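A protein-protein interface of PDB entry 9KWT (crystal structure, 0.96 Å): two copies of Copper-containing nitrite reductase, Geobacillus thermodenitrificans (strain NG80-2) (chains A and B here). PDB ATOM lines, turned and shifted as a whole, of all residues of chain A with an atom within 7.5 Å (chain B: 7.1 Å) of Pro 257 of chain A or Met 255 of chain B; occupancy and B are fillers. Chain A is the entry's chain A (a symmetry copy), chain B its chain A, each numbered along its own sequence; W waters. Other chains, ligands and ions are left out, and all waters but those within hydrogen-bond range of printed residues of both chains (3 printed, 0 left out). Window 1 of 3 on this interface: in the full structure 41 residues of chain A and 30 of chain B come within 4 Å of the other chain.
Printed residues of chain A that touch a printed residue of chain B: Asn 218, Asn 223, Val 225, Asp 241, Met 255, Pro 257, Ala 258, Ser 259 and Gly 261. Along chain A the printed residues that touch a printed residue of chain B span positions 218 to 261. Hydrophobic or aromatic side chains of chain B that line the printed part of chain A: Val 225, Met 251, Met 255 and His 279. Among the printed residues, 20 pairs touch across the chains. Among the printed residues, no Asp or Glu carboxylate lies within 4 Å of a Lys or Arg side-chain nitrogen of the other chain.
Val 225 of chain A touches its own counterpart, Val 225 of chain B. Val 225 of chain A touches Met 255 of chain B, but with the chains exchanged Met 255 of chain A does not touch Val 225 of chain B (6.7 Å). Met 255 of chain B touches its own counterpart, Met 255 of chain A. Pro 257 of chain A touches Met 255 of chain B, but with the chains exchanged Met 255 of chain A does not touch Pro 257 of chain B (7.9 Å). Of the 20 pairs that touch across the chains among the printed residues, 2 have their exchanged pair printed and touching as well.
Water W2 bridges the backbone carbonyl oxygen (O) of Asn 223 of chain A (2.7 Å) and the side-chain amide nitrogen (NE2) of Gln 280 of chain B (3.3 Å). Water W1 lies within hydrogen-bond range of a ring nitrogen (ND1) of His 279 of chain B (2.8 Å) and the backbone carbonyl oxygen of Val 220 of chain A (2.9 Å). Water W3 lies within hydrogen-bond range of the backbone carbonyl oxygen of Thr 253 of chain B and the side-chain carboxylate of Asp 241 of chain A.
OG of Ser 227 of chain B sits at hydrogen-bond distance from N of Ala 258 of chain A, at 3.0 Å. N of Gln 252 of chain B is in hydrogen-bond range of OD2 of Asp 241 of chain A (2.7 Å). O of Ser 259 of chain A lies close to NE2 of Gln 252 of chain B (3.2 Å). OG1 of Thr 253 of chain B sits at hydrogen-bond distance from OG of Ser 259 of chain A, at 2.7 Å. OD2 of Asp 241 of chain A lies close to SD of Met 251 of chain B, 3.8 Å away.
Among the printed residues, pairs that only touch across the chains: Pro 257 of chain A with Ser 227 of chain B, Asn 223 of chain A with Gln 280 of chain B, Ala 258 of chain A with His 279 of chain B, Ser 259 of chain A with His 279 of chain B, Asn 218 of chain A with Gln 252 of chain B, Pro 257 of chain A with Met 255 of chain B, Ala 258 of chain A with Thr 253 of chain B, Asp 241 of chain A with Thr 253 of chain B, Gly 261 of chain A with Gln 252 of chain B, Pro 257 of chain A with Thr 253 of chain B, Ala 258 of chain A with Gln 280 of chain B, Met 255 of chain A with Met 255 of chain B, Val 225 of chain A with Val 225 of chain B, Val 225 of chain A with Gln 280 of chain B and Val 225 of chain A with Met 255 of chain B.
Pro 257 of chain A touches three residues of chain B. Of chain A, only Val 225, Met 255 and Pro 257 come within 4 Å of Met 255 of chain B. Of the printed residues of chain B, Ser 259 of chain A touches Gln 252 (3.1 Å), Thr 253 (2.7 Å) and His 279 (3.6 Å). Printed residues of chain A within 4 Å of Gln 252 of chain B: Asn 218, Asp 241, Ser 259 and Gly 261. Printed residues of chain B within 4 Å of Gly 261 of chain A: Gln 252. Gly 221 of chain A touches none of the printed residues of chain B. Pro 257 of chain B touches none of the printed residues of chain A. The nearest residue of chain B that does not touch Pro 257 of chain A is Val 254 of chain B (4.8 Å). The nearest residue of chain A that does not touch Met 255 of chain B is Leu 256 of chain A (4.3 Å).
The backbone carbonyl oxygen (O) of Val 225 of chain B is in hydrogen-bond range of the side-chain amide nitrogen (NE2) of Gln 280 of chain B, 3.1 Å away. N of His 279 of chain B sits at hydrogen-bond distance from O of Ser 227 of chain B (2.7 Å). The side-chain amide oxygen of Gln 280 of chain B is in hydrogen-bond range of the side-chain hydroxyl of Ser 227 of chain B, at 2.7 Å. The backbone carbonyl oxygen (O) of Ser 259 of chain A lies within hydrogen-bond range of the side-chain amide nitrogen (ND2) of Asn 218 of chain A (3.0 Å). The side-chain amide nitrogen (ND2) of Asn 218 of chain A sits close to the backbone carbonyl oxygen (O) of Gly 260 of chain A. The backbone NH (N) of Asp 241 of chain A lies within hydrogen-bond range of the backbone carbonyl oxygen (O) of Gly 261 of chain A.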
ATOM      1  N   ASN A 218     -10.508   0.909  23.159  1.00  0.00           N
ATOM      2  CA  ASN A 218     -11.846   1.468  23.193  1.00  0.00           C
ATOM      3  C   ASN A 218     -12.836   0.341  22.975  1.00  0.00           C
ATOM      4  O   ASN A 218     -12.621  -0.531  22.128  1.00  0.00           O
ATOM      5  CB  ASN A 218     -12.033   2.586  22.154  1.00  0.00           C
ATOM      6  CG  ASN A 218     -13.316   3.366  22.367  1.00  0.00           C
ATOM      7  OD1 ASN A 218     -14.413   2.875  22.108  1.00  0.00           O
ATOM      8  ND2 ASN A 218     -13.185   4.592  22.872  1.00  0.00           N
ATOM      9  N   ASN A 219     -13.911   0.375  23.745  1.00  0.00           N
ATOM     10  CA  ASN A 219     -15.055  -0.512  23.566  1.00  0.00           C
ATOM     11  C   ASN A 219     -16.115   0.260  22.806  1.00  0.00           C
ATOM     12  O   ASN A 219     -16.802   1.097  23.391  1.00  0.00           O
ATOM     13  CB  ASN A 219     -15.599  -0.903  24.930  1.00  0.00           C
ATOM     14  CG  ASN A 219     -16.950  -1.546  24.825  1.00  0.00           C
ATOM     15  OD1 ASN A 219     -17.225  -2.248  23.835  1.00  0.00           O
ATOM     16  ND2 ASN A 219     -17.797  -1.323  25.817  1.00  0.00           N
ATOM     17  N   VAL A 220     -16.257  -0.011  21.508  1.00  0.00           N
ATOM     18  CA  VAL A 220     -17.202   0.748  20.694  1.00  0.00           C
ATOM     19  C   VAL A 220     -18.628   0.228  20.794  1.00  0.00           C
ATOM     20  O   VAL A 220     -19.556   0.868  20.280  1.00  0.00           O
ATOM     21  CB  VAL A 220     -16.755   0.858  19.222  1.00  0.00           C
ATOM     22  CG1 VAL A 220     -15.410   1.579  19.119  1.00  0.00           C
ATOM     23  CG2 VAL A 220     -16.727  -0.494  18.531  1.00  0.00           C
ATOM     24  N   GLY A 221     -18.852  -0.899  21.457  1.00  0.00           N
ATOM     25  CA  GLY A 221     -20.195  -1.410  21.578  1.00  0.00           C
ATOM     26  C   GLY A 221     -20.653  -2.153  20.334  1.00  0.00           C
ATOM     27  O   GLY A 221     -19.898  -2.937  19.765  1.00  0.00           O
ATOM     28  N   ASN A 223     -23.595  -1.940  22.211  1.00  0.00           N
ATOM     29  CA  ASN A 223     -24.510  -2.051  23.336  1.00  0.00           C
ATOM     30  C   ASN A 223     -23.900  -2.425  24.663  1.00  0.00           C
ATOM     31  O   ASN A 223     -24.495  -2.108  25.700  1.00  0.00           O
ATOM     32  CB  ASN A 223     -25.584  -3.088  23.014  1.00  0.00           C
ATOM     33  CG  ASN A 223     -26.407  -2.717  21.806  1.00  0.00           C
ATOM     34  OD1 ASN A 223     -26.594  -1.530  21.499  1.00  0.00           O
ATOM     35  ND2 ASN A 223     -26.910  -3.717  21.111  1.00  0.00           N
ATOM     36  N   GLU A 224     -22.788  -3.140  24.673  1.00  0.00           N
ATOM     37  CA  GLU A 224     -22.279  -3.728  25.902  1.00  0.00           C
ATOM     38  C   GLU A 224     -21.185  -2.864  26.508  1.00  0.00           C
ATOM     39  O   GLU A 224     -20.464  -2.158  25.795  1.00  0.00           O
ATOM     40  CB  GLU A 224     -21.688  -5.114  25.642  1.00  0.00           C
ATOM     41  CG  GLU A 224     -22.641  -6.118  25.004  1.00  0.00           C
ATOM     42  CD  GLU A 224     -23.770  -6.614  25.883  1.00  0.00           C
ATOM     43  OE1 GLU A 224     -23.751  -6.446  27.107  1.00  0.00           O
ATOM     44  OE2 GLU A 224     -24.653  -7.318  25.341  1.00  0.00           O
ATOM     45  N   VAL A 225     -21.037  -2.976  27.832  1.00  0.00           N
ATOM     46  CA  VAL A 225     -19.872  -2.466  28.543  1.00  0.00           C
ATOM     47  C   VAL A 225     -18.801  -3.553  28.527  1.00  0.00           C
ATOM     48  O   VAL A 225     -19.081  -4.711  28.190  1.00  0.00           O
ATOM     49  CB  VAL A 225     -20.237  -1.994  29.961  1.00  0.00           C
ATOM     50  CG1 VAL A 225     -21.331  -0.940  29.883  1.00  0.00           C
ATOM     51  CG2 VAL A 225     -20.678  -3.147  30.864  1.00  0.00           C
ATOM     52  N   SER A 226     -17.564  -3.189  28.868  1.00  0.00           N
ATOM     53  CA  SER A 226     -16.432  -4.108  28.806  1.00  0.00           C
ATOM     54  C   SER A 226     -15.661  -4.097  30.115  1.00  0.00           C
ATOM     55  O   SER A 226     -15.434  -3.046  30.712  1.00  0.00           O
ATOM     56  CB  SER A 226     -15.488  -3.711  27.665  1.00  0.00           C
ATOM     57  OG  SER A 226     -14.324  -4.511  27.649  1.00  0.00           O
ATOM     58  N   LEU A 240      -8.008   6.985  32.164  1.00  0.00           N
ATOM     59  CA  LEU A 240      -9.355   6.819  31.640  1.00  0.00           C
ATOM     60  C   LEU A 240      -9.589   7.782  30.487  1.00  0.00           C
ATOM     61  O   LEU A 240      -9.233   8.970  30.553  1.00  0.00           O
ATOM     62  CB  LEU A 240     -10.397   7.039  32.729  1.00  0.00           C
ATOM     63  CG  LEU A 240     -10.336   6.079  33.922  1.00  0.00           C
ATOM     64  CD1 LEU A 240     -11.422   6.452  34.911  1.00  0.00           C
ATOM     65  CD2 LEU A 240     -10.487   4.627  33.499  1.00  0.00           C
ATOM     66  N   ASP A 241     -10.162   7.246  29.413  1.00  0.00           N
ATOM     67  CA  ASP A 241     -10.361   7.925  28.140  1.00  0.00           C
ATOM     68  C   ASP A 241      -9.053   8.410  27.524  1.00  0.00           C
ATOM     69  O   ASP A 241      -9.077   9.159  26.547  1.00  0.00           O
ATOM     70  CB  ASP A 241     -11.435   9.015  28.190  1.00  0.00           C
ATOM     71  CG  ASP A 241     -12.830   8.465  27.922  1.00  0.00           C
ATOM     72  OD1 ASP A 241     -12.923   7.360  27.330  1.00  0.00           O
ATOM     73  OD2 ASP A 241     -13.806   9.155  28.287  1.00  0.00           O
ATOM     74  N   VAL A 254     -10.340  -2.986  33.911  1.00  0.00           N
ATOM     75  CA  VAL A 254     -10.798  -1.626  33.649  1.00  0.00           C
ATOM     76  C   VAL A 254     -12.218  -1.670  33.085  1.00  0.00           C
ATOM     77  O   VAL A 254     -12.456  -2.239  32.018  1.00  0.00           O
ATOM     78  CB  VAL A 254      -9.842  -0.893  32.698  1.00  0.00           C
ATOM     79  CG1 VAL A 254     -10.374   0.491  32.358  1.00  0.00           C
ATOM     80  CG2 VAL A 254      -8.452  -0.786  33.325  1.00  0.00           C
ATOM     81  N   MET A 255     -13.150  -1.040  33.789  1.00  0.00           N
ATOM     82  CA  MET A 255     -14.539  -0.921  33.355  1.00  0.00           C
ATOM     83  C   MET A 255     -14.641   0.141  32.264  1.00  0.00           C
ATOM     84  O   MET A 255     -14.337   1.309  32.515  1.00  0.00           O
ATOM     85  CB  MET A 255     -15.348  -0.457  34.571  1.00  0.00           C
ATOM     86  CG  MET A 255     -16.828  -0.226  34.476  1.00  0.00           C
ATOM     87  SD  MET A 255     -17.872  -1.715  34.438  1.00  0.00           S
ATOM     88  CE  MET A 255     -17.681  -2.267  32.751  1.00  0.00           C
ATOM     89  N   LEU A 256     -15.088  -0.254  31.068  1.00  0.00           N
ATOM     90  CA  LEU A 256     -15.286   0.674  29.960  1.00  0.00           C
ATOM     91  C   LEU A 256     -16.765   0.762  29.633  1.00  0.00           C
ATOM     92  O   LEU A 256     -17.387  -0.271  29.319  1.00  0.00           O
ATOM     93  CB  LEU A 256     -14.539   0.203  28.719  1.00  0.00           C
ATOM     94  CG  LEU A 256     -13.028   0.062  28.826  1.00  0.00           C
ATOM     95  CD1 LEU A 256     -12.480  -0.613  27.591  1.00  0.00           C
ATOM     96  CD2 LEU A 256     -12.352   1.410  29.056  1.00  0.00           C
ATOM     97  N   PRO A 257     -17.361   1.949  29.648  1.00  0.00           N
ATOM     98  CA  PRO A 257     -18.716   2.085  29.122  1.00  0.00           C
ATOM     99  C   PRO A 257     -18.717   1.793  27.629  1.00  0.00           C
ATOM    100  O   PRO A 257     -17.665   1.668  26.992  1.00  0.00           O
ATOM    101  CB  PRO A 257     -19.068   3.545  29.422  1.00  0.00           C
ATOM    102  CG  PRO A 257     -17.732   4.259  29.438  1.00  0.00           C
ATOM    103  CD  PRO A 257     -16.774   3.249  30.018  1.00  0.00           C
ATOM    104  N   ALA A 258     -19.914   1.714  27.051  1.00  0.00           N
ATOM    105  CA  ALA A 258     -20.006   1.720  25.590  1.00  0.00           C
ATOM    106  C   ALA A 258     -19.492   3.063  25.087  1.00  0.00           C
ATOM    107  O   ALA A 258     -19.964   4.107  25.552  1.00  0.00           O
ATOM    108  CB  ALA A 258     -21.445   1.480  25.151  1.00  0.00           C
ATOM    109  N   SER A 259     -18.530   3.015  24.162  1.00  0.00           N
ATOM    110  CA  SER A 259     -17.698   4.098  23.629  1.00  0.00           C
ATOM    111  C   SER A 259     -16.538   4.473  24.534  1.00  0.00           C
ATOM    112  O   SER A 259     -15.789   5.399  24.200  1.00  0.00           O
ATOM    113  CB  SER A 259     -18.471   5.367  23.238  1.00  0.00           C
ATOM    114  OG  SER A 259     -18.897   6.147  24.338  1.00  0.00           O
ATOM    115  N   GLY A 260     -16.359   3.796  25.660  1.00  0.00           N
ATOM    116  CA  GLY A 260     -15.310   4.159  26.588  1.00  0.00           C
ATOM    117  C   GLY A 260     -13.931   3.744  26.116  1.00  0.00           C
ATOM    118  O   GLY A 260     -13.722   2.649  25.583  1.00  0.00           O
ATOM    119  N   GLY A 261     -12.964   4.620  26.390  1.00  0.00           N
ATOM    120  CA  GLY A 261     -11.581   4.379  26.054  1.00  0.00           C
ATOM    121  C   GLY A 261     -10.673   4.383  27.276  1.00  0.00           C
ATOM    122  O   GLY A 261     -11.057   4.785  28.377  1.00  0.00           O
ATOM    123  N   ASN B 219     -28.557   7.983  36.847  1.00  0.00           N
ATOM    124  CA  ASN B 219     -29.195   6.833  36.216  1.00  0.00           C
ATOM    125  C   ASN B 219     -29.877   6.035  37.309  1.00  0.00           C
ATOM    126  O   ASN B 219     -29.208   5.311  38.048  1.00  0.00           O
ATOM    127  CB  ASN B 219     -28.131   5.975  35.554  1.00  0.00           C
ATOM    128  CG  ASN B 219     -28.666   4.629  35.166  1.00  0.00           C
ATOM    129  OD1 ASN B 219     -29.852   4.516  34.803  1.00  0.00           O
ATOM    130  ND2 ASN B 219     -27.825   3.608  35.232  1.00  0.00           N
ATOM    131  N   VAL B 225     -27.016  -0.122  33.583  1.00  0.00           N
ATOM    132  CA  VAL B 225     -25.985   0.900  33.709  1.00  0.00           C
ATOM    133  C   VAL B 225     -26.122   1.852  32.523  1.00  0.00           C
ATOM    134  O   VAL B 225     -26.831   1.554  31.552  1.00  0.00           O
ATOM    135  CB  VAL B 225     -24.583   0.278  33.828  1.00  0.00           C
ATOM    136  CG1 VAL B 225     -24.549  -0.678  35.011  1.00  0.00           C
ATOM    137  CG2 VAL B 225     -24.156  -0.447  32.550  1.00  0.00           C
ATOM    138  N   SER B 226     -25.469   3.012  32.599  1.00  0.00           N
ATOM    139  CA  SER B 226     -25.588   4.047  31.578  1.00  0.00           C
ATOM    140  C   SER B 226     -24.215   4.513  31.124  1.00  0.00           C
ATOM    141  O   SER B 226     -23.305   4.694  31.931  1.00  0.00           O
ATOM    142  CB  SER B 226     -26.369   5.247  32.128  1.00  0.00           C
ATOM    143  OG  SER B 226     -26.404   6.313  31.203  1.00  0.00           O
ATOM    144  N   SER B 227     -24.093   4.742  29.819  1.00  0.00           N
ATOM    145  CA  SER B 227     -22.848   5.200  29.199  1.00  0.00           C
ATOM    146  C   SER B 227     -23.111   6.633  28.701  1.00  0.00           C
ATOM    147  O   SER B 227     -23.412   6.870  27.529  1.00  0.00           O
ATOM    148  CB  SER B 227     -22.520   4.251  28.053  1.00  0.00           C
ATOM    149  OG  SER B 227     -22.141   2.970  28.549  1.00  0.00           O
ATOM    150  N   PHE B 228     -23.055   7.598  29.615  1.00  0.00           N
ATOM    151  CA  PHE B 228     -23.624   8.915  29.345  1.00  0.00           C
ATOM    152  C   PHE B 228     -22.692   9.754  28.467  1.00  0.00           C
ATOM    153  O   PHE B 228     -21.511   9.917  28.784  1.00  0.00           O
ATOM    154  CB  PHE B 228     -23.903   9.624  30.669  1.00  0.00           C
ATOM    155  CG  PHE B 228     -24.624  10.919  30.496  1.00  0.00           C
ATOM    156  CD1 PHE B 228     -25.990  10.939  30.332  1.00  0.00           C
ATOM    157  CD2 PHE B 228     -23.933  12.117  30.434  1.00  0.00           C
ATOM    158  CE1 PHE B 228     -26.663  12.135  30.138  1.00  0.00           C
ATOM    159  CE2 PHE B 228     -24.603  13.319  30.246  1.00  0.00           C
ATOM    160  CZ  PHE B 228     -25.967  13.324  30.107  1.00  0.00           C
ATOM    161  N   LEU B 240     -17.633  12.459  40.019  1.00  0.00           N
ATOM    162  CA  LEU B 240     -18.421  11.249  40.197  1.00  0.00           C
ATOM    163  C   LEU B 240     -19.264  11.355  41.459  1.00  0.00           C
ATOM    164  O   LEU B 240     -18.787  11.789  42.520  1.00  0.00           O
ATOM    165  CB  LEU B 240     -17.527  10.018  40.263  1.00  0.00           C
ATOM    166  CG  LEU B 240     -16.678   9.735  39.018  1.00  0.00           C
ATOM    167  CD1 LEU B 240     -15.841   8.497  39.264  1.00  0.00           C
ATOM    168  CD2 LEU B 240     -17.529   9.557  37.772  1.00  0.00           C
ATOM    169  N   MET B 251     -13.441  13.521  29.652  1.00  0.00           N
ATOM    170  CA  MET B 251     -14.098  12.244  29.388  1.00  0.00           C
ATOM    171  C   MET B 251     -15.051  12.378  28.207  1.00  0.00           C
ATOM    172  O   MET B 251     -15.829  13.331  28.133  1.00  0.00           O
ATOM    173  CB  MET B 251     -14.897  11.791  30.610  1.00  0.00           C
ATOM    174  CG  MET B 251     -14.051  11.591  31.863  1.00  0.00           C
ATOM    175  SD  MET B 251     -12.952  10.151  31.812  1.00  0.00           S
ATOM    176  CE  MET B 251     -14.149   8.815  31.735  1.00  0.00           C
ATOM    177  N   GLN B 252     -15.006  11.407  27.296  1.00  0.00           N
ATOM    178  CA  GLN B 252     -16.014  11.360  26.240  1.00  0.00           C
ATOM    179  C   GLN B 252     -17.362  10.886  26.767  1.00  0.00           C
ATOM    180  O   GLN B 252     -18.412  11.363  26.323  1.00  0.00           O
ATOM    181  CB  GLN B 252     -15.556  10.498  25.056  1.00  0.00           C
ATOM    182  CG  GLN B 252     -15.540   8.988  25.260  1.00  0.00           C
ATOM    183  CD  GLN B 252     -14.739   8.323  24.177  1.00  0.00           C
ATOM    184  OE1 GLN B 252     -15.111   8.356  22.992  1.00  0.00           O
ATOM    185  NE2 GLN B 252     -13.607   7.759  24.564  1.00  0.00           N
ATOM    186  N   THR B 253     -17.329   9.928  27.691  1.00  0.00           N
ATOM    187  CA  THR B 253     -18.495   9.174  28.124  1.00  0.00           C
ATOM    188  C   THR B 253     -18.293   8.830  29.590  1.00  0.00           C
ATOM    189  O   THR B 253     -17.189   8.448  29.985  1.00  0.00           O
ATOM    190  CB  THR B 253     -18.636   7.914  27.267  1.00  0.00           C
ATOM    191  OG1 THR B 253     -18.898   8.374  25.940  1.00  0.00           O
ATOM    192  CG2 THR B 253     -19.776   7.010  27.746  1.00  0.00           C
ATOM    193  N   VAL B 254     -19.349   8.957  30.391  1.00  0.00           N
ATOM    194  CA  VAL B 254     -19.280   8.685  31.823  1.00  0.00           C
ATOM    195  C   VAL B 254     -20.084   7.424  32.138  1.00  0.00           C
ATOM    196  O   VAL B 254     -21.295   7.374  31.918  1.00  0.00           O
ATOM    197  CB  VAL B 254     -19.782   9.884  32.639  1.00  0.00           C
ATOM    198  CG1 VAL B 254     -19.791   9.560  34.125  1.00  0.00           C
ATOM    199  CG2 VAL B 254     -18.906  11.108  32.372  1.00  0.00           C
ATOM    200  N   MET B 255     -19.410   6.418  32.682  1.00  0.00           N
ATOM    201  CA  MET B 255     -20.038   5.172  33.113  1.00  0.00           C
ATOM    202  C   MET B 255     -20.768   5.401  34.433  1.00  0.00           C
ATOM    203  O   MET B 255     -20.133   5.742  35.433  1.00  0.00           O
ATOM    204  CB  MET B 255     -18.909   4.161  33.343  1.00  0.00           C
ATOM    205  CG  MET B 255     -19.203   2.762  33.803  1.00  0.00           C
ATOM    206  SD  MET B 255     -19.867   1.628  32.545  1.00  0.00           S
ATOM    207  CE  MET B 255     -21.577   2.133  32.448  1.00  0.00           C
ATOM    208  N   LEU B 256     -22.088   5.192  34.444  1.00  0.00           N
ATOM    209  CA  LEU B 256     -22.891   5.320  35.655  1.00  0.00           C
ATOM    210  C   LEU B 256     -23.444   3.961  36.040  1.00  0.00           C
ATOM    211  O   LEU B 256     -24.156   3.335  35.231  1.00  0.00           O
ATOM    212  CB  LEU B 256     -24.057   6.277  35.434  1.00  0.00           C
ATOM    213  CG  LEU B 256     -23.719   7.709  35.052  1.00  0.00           C
ATOM    214  CD1 LEU B 256     -24.976   8.454  34.663  1.00  0.00           C
ATOM    215  CD2 LEU B 256     -22.983   8.433  36.176  1.00  0.00           C
ATOM    216  N   PRO B 257     -23.191   3.481  37.252  1.00  0.00           N
ATOM    217  CA  PRO B 257     -23.894   2.288  37.719  1.00  0.00           C
ATOM    218  C   PRO B 257     -25.381   2.587  37.843  1.00  0.00           C
ATOM    219  O   PRO B 257     -25.821   3.738  37.744  1.00  0.00           O
ATOM    220  CB  PRO B 257     -23.249   2.006  39.079  1.00  0.00           C
ATOM    221  CG  PRO B 257     -22.779   3.363  39.561  1.00  0.00           C
ATOM    222  CD  PRO B 257     -22.355   4.081  38.306  1.00  0.00           C
ATOM    223  N   GLY B 260     -26.206   5.480  39.941  1.00  0.00           N
ATOM    224  CA  GLY B 260     -25.036   6.329  39.885  1.00  0.00           C
ATOM    225  C   GLY B 260     -25.347   7.737  39.418  1.00  0.00           C
ATOM    226  O   GLY B 260     -26.130   7.962  38.490  1.00  0.00           O
ATOM    227  N   GLY B 261     -24.655   8.693  40.039  1.00  0.00           N
ATOM    228  CA  GLY B 261     -24.787  10.090  39.700  1.00  0.00           C
ATOM    229  C   GLY B 261     -23.473  10.707  39.244  1.00  0.00           C
ATOM    230  O   GLY B 261     -22.392  10.129  39.385  1.00  0.00           O
ATOM    231  N   ALA B 262     -23.586  11.919  38.713  1.00  0.00           N
ATOM    232  CA  ALA B 262     -22.410  12.699  38.376  1.00  0.00           C
ATOM    233  C   ALA B 262     -22.825  14.151  38.196  1.00  0.00           C
ATOM    234  O   ALA B 262     -23.982  14.459  37.918  1.00  0.00           O
ATOM    235  CB  ALA B 262     -21.728  12.208  37.099  1.00  0.00           C
ATOM    236  N   HIS B 279     -24.829   5.748  25.463  1.00  0.00           N
ATOM    237  CA  HIS B 279     -24.145   5.205  24.298  1.00  0.00           C
ATOM    238  C   HIS B 279     -24.294   3.702  24.170  1.00  0.00           C
ATOM    239  O   HIS B 279     -23.755   3.120  23.224  1.00  0.00           O
ATOM    240  CB  HIS B 279     -22.665   5.609  24.296  1.00  0.00           C
ATOM    241  CG  HIS B 279     -22.167   5.983  22.942  1.00  0.00           C
ATOM    242  ND1 HIS B 279     -21.879   5.064  21.962  1.00  0.00           N
ATOM    243  CD2 HIS B 279     -21.939   7.197  22.397  1.00  0.00           C
ATOM    244  CE1 HIS B 279     -21.500   5.708  20.869  1.00  0.00           C
ATOM    245  NE2 HIS B 279     -21.528   7.007  21.104  1.00  0.00           N
ATOM    246  N   GLN B 280     -25.013   3.076  25.102  1.00  0.00           N
ATOM    247  CA  GLN B 280     -25.531   1.729  24.915  1.00  0.00           C
ATOM    248  C   GLN B 280     -26.694   1.885  23.947  1.00  0.00           C
ATOM    249  O   GLN B 280     -27.793   2.296  24.335  1.00  0.00           O
ATOM    250  CB  GLN B 280     -25.924   1.152  26.266  1.00  0.00           C
ATOM    251  CG  GLN B 280     -24.685   0.886  27.126  1.00  0.00           C
ATOM    252  CD  GLN B 280     -24.958   0.851  28.617  1.00  0.00           C
ATOM    253  OE1 GLN B 280     -24.347   1.604  29.386  1.00  0.00           O
ATOM    254  NE2 GLN B 280     -25.859  -0.014  29.042  1.00  0.00           N
HETATM  255  O   HOH W   1     -21.746   2.393  21.301  1.00  0.00           O
HETATM  256  O   HOH W   2     -27.020  -1.989  26.733  1.00  0.00           O
HETATM  257  O   HOH W   3     -15.409   6.665  28.710  1.00  0.00           O
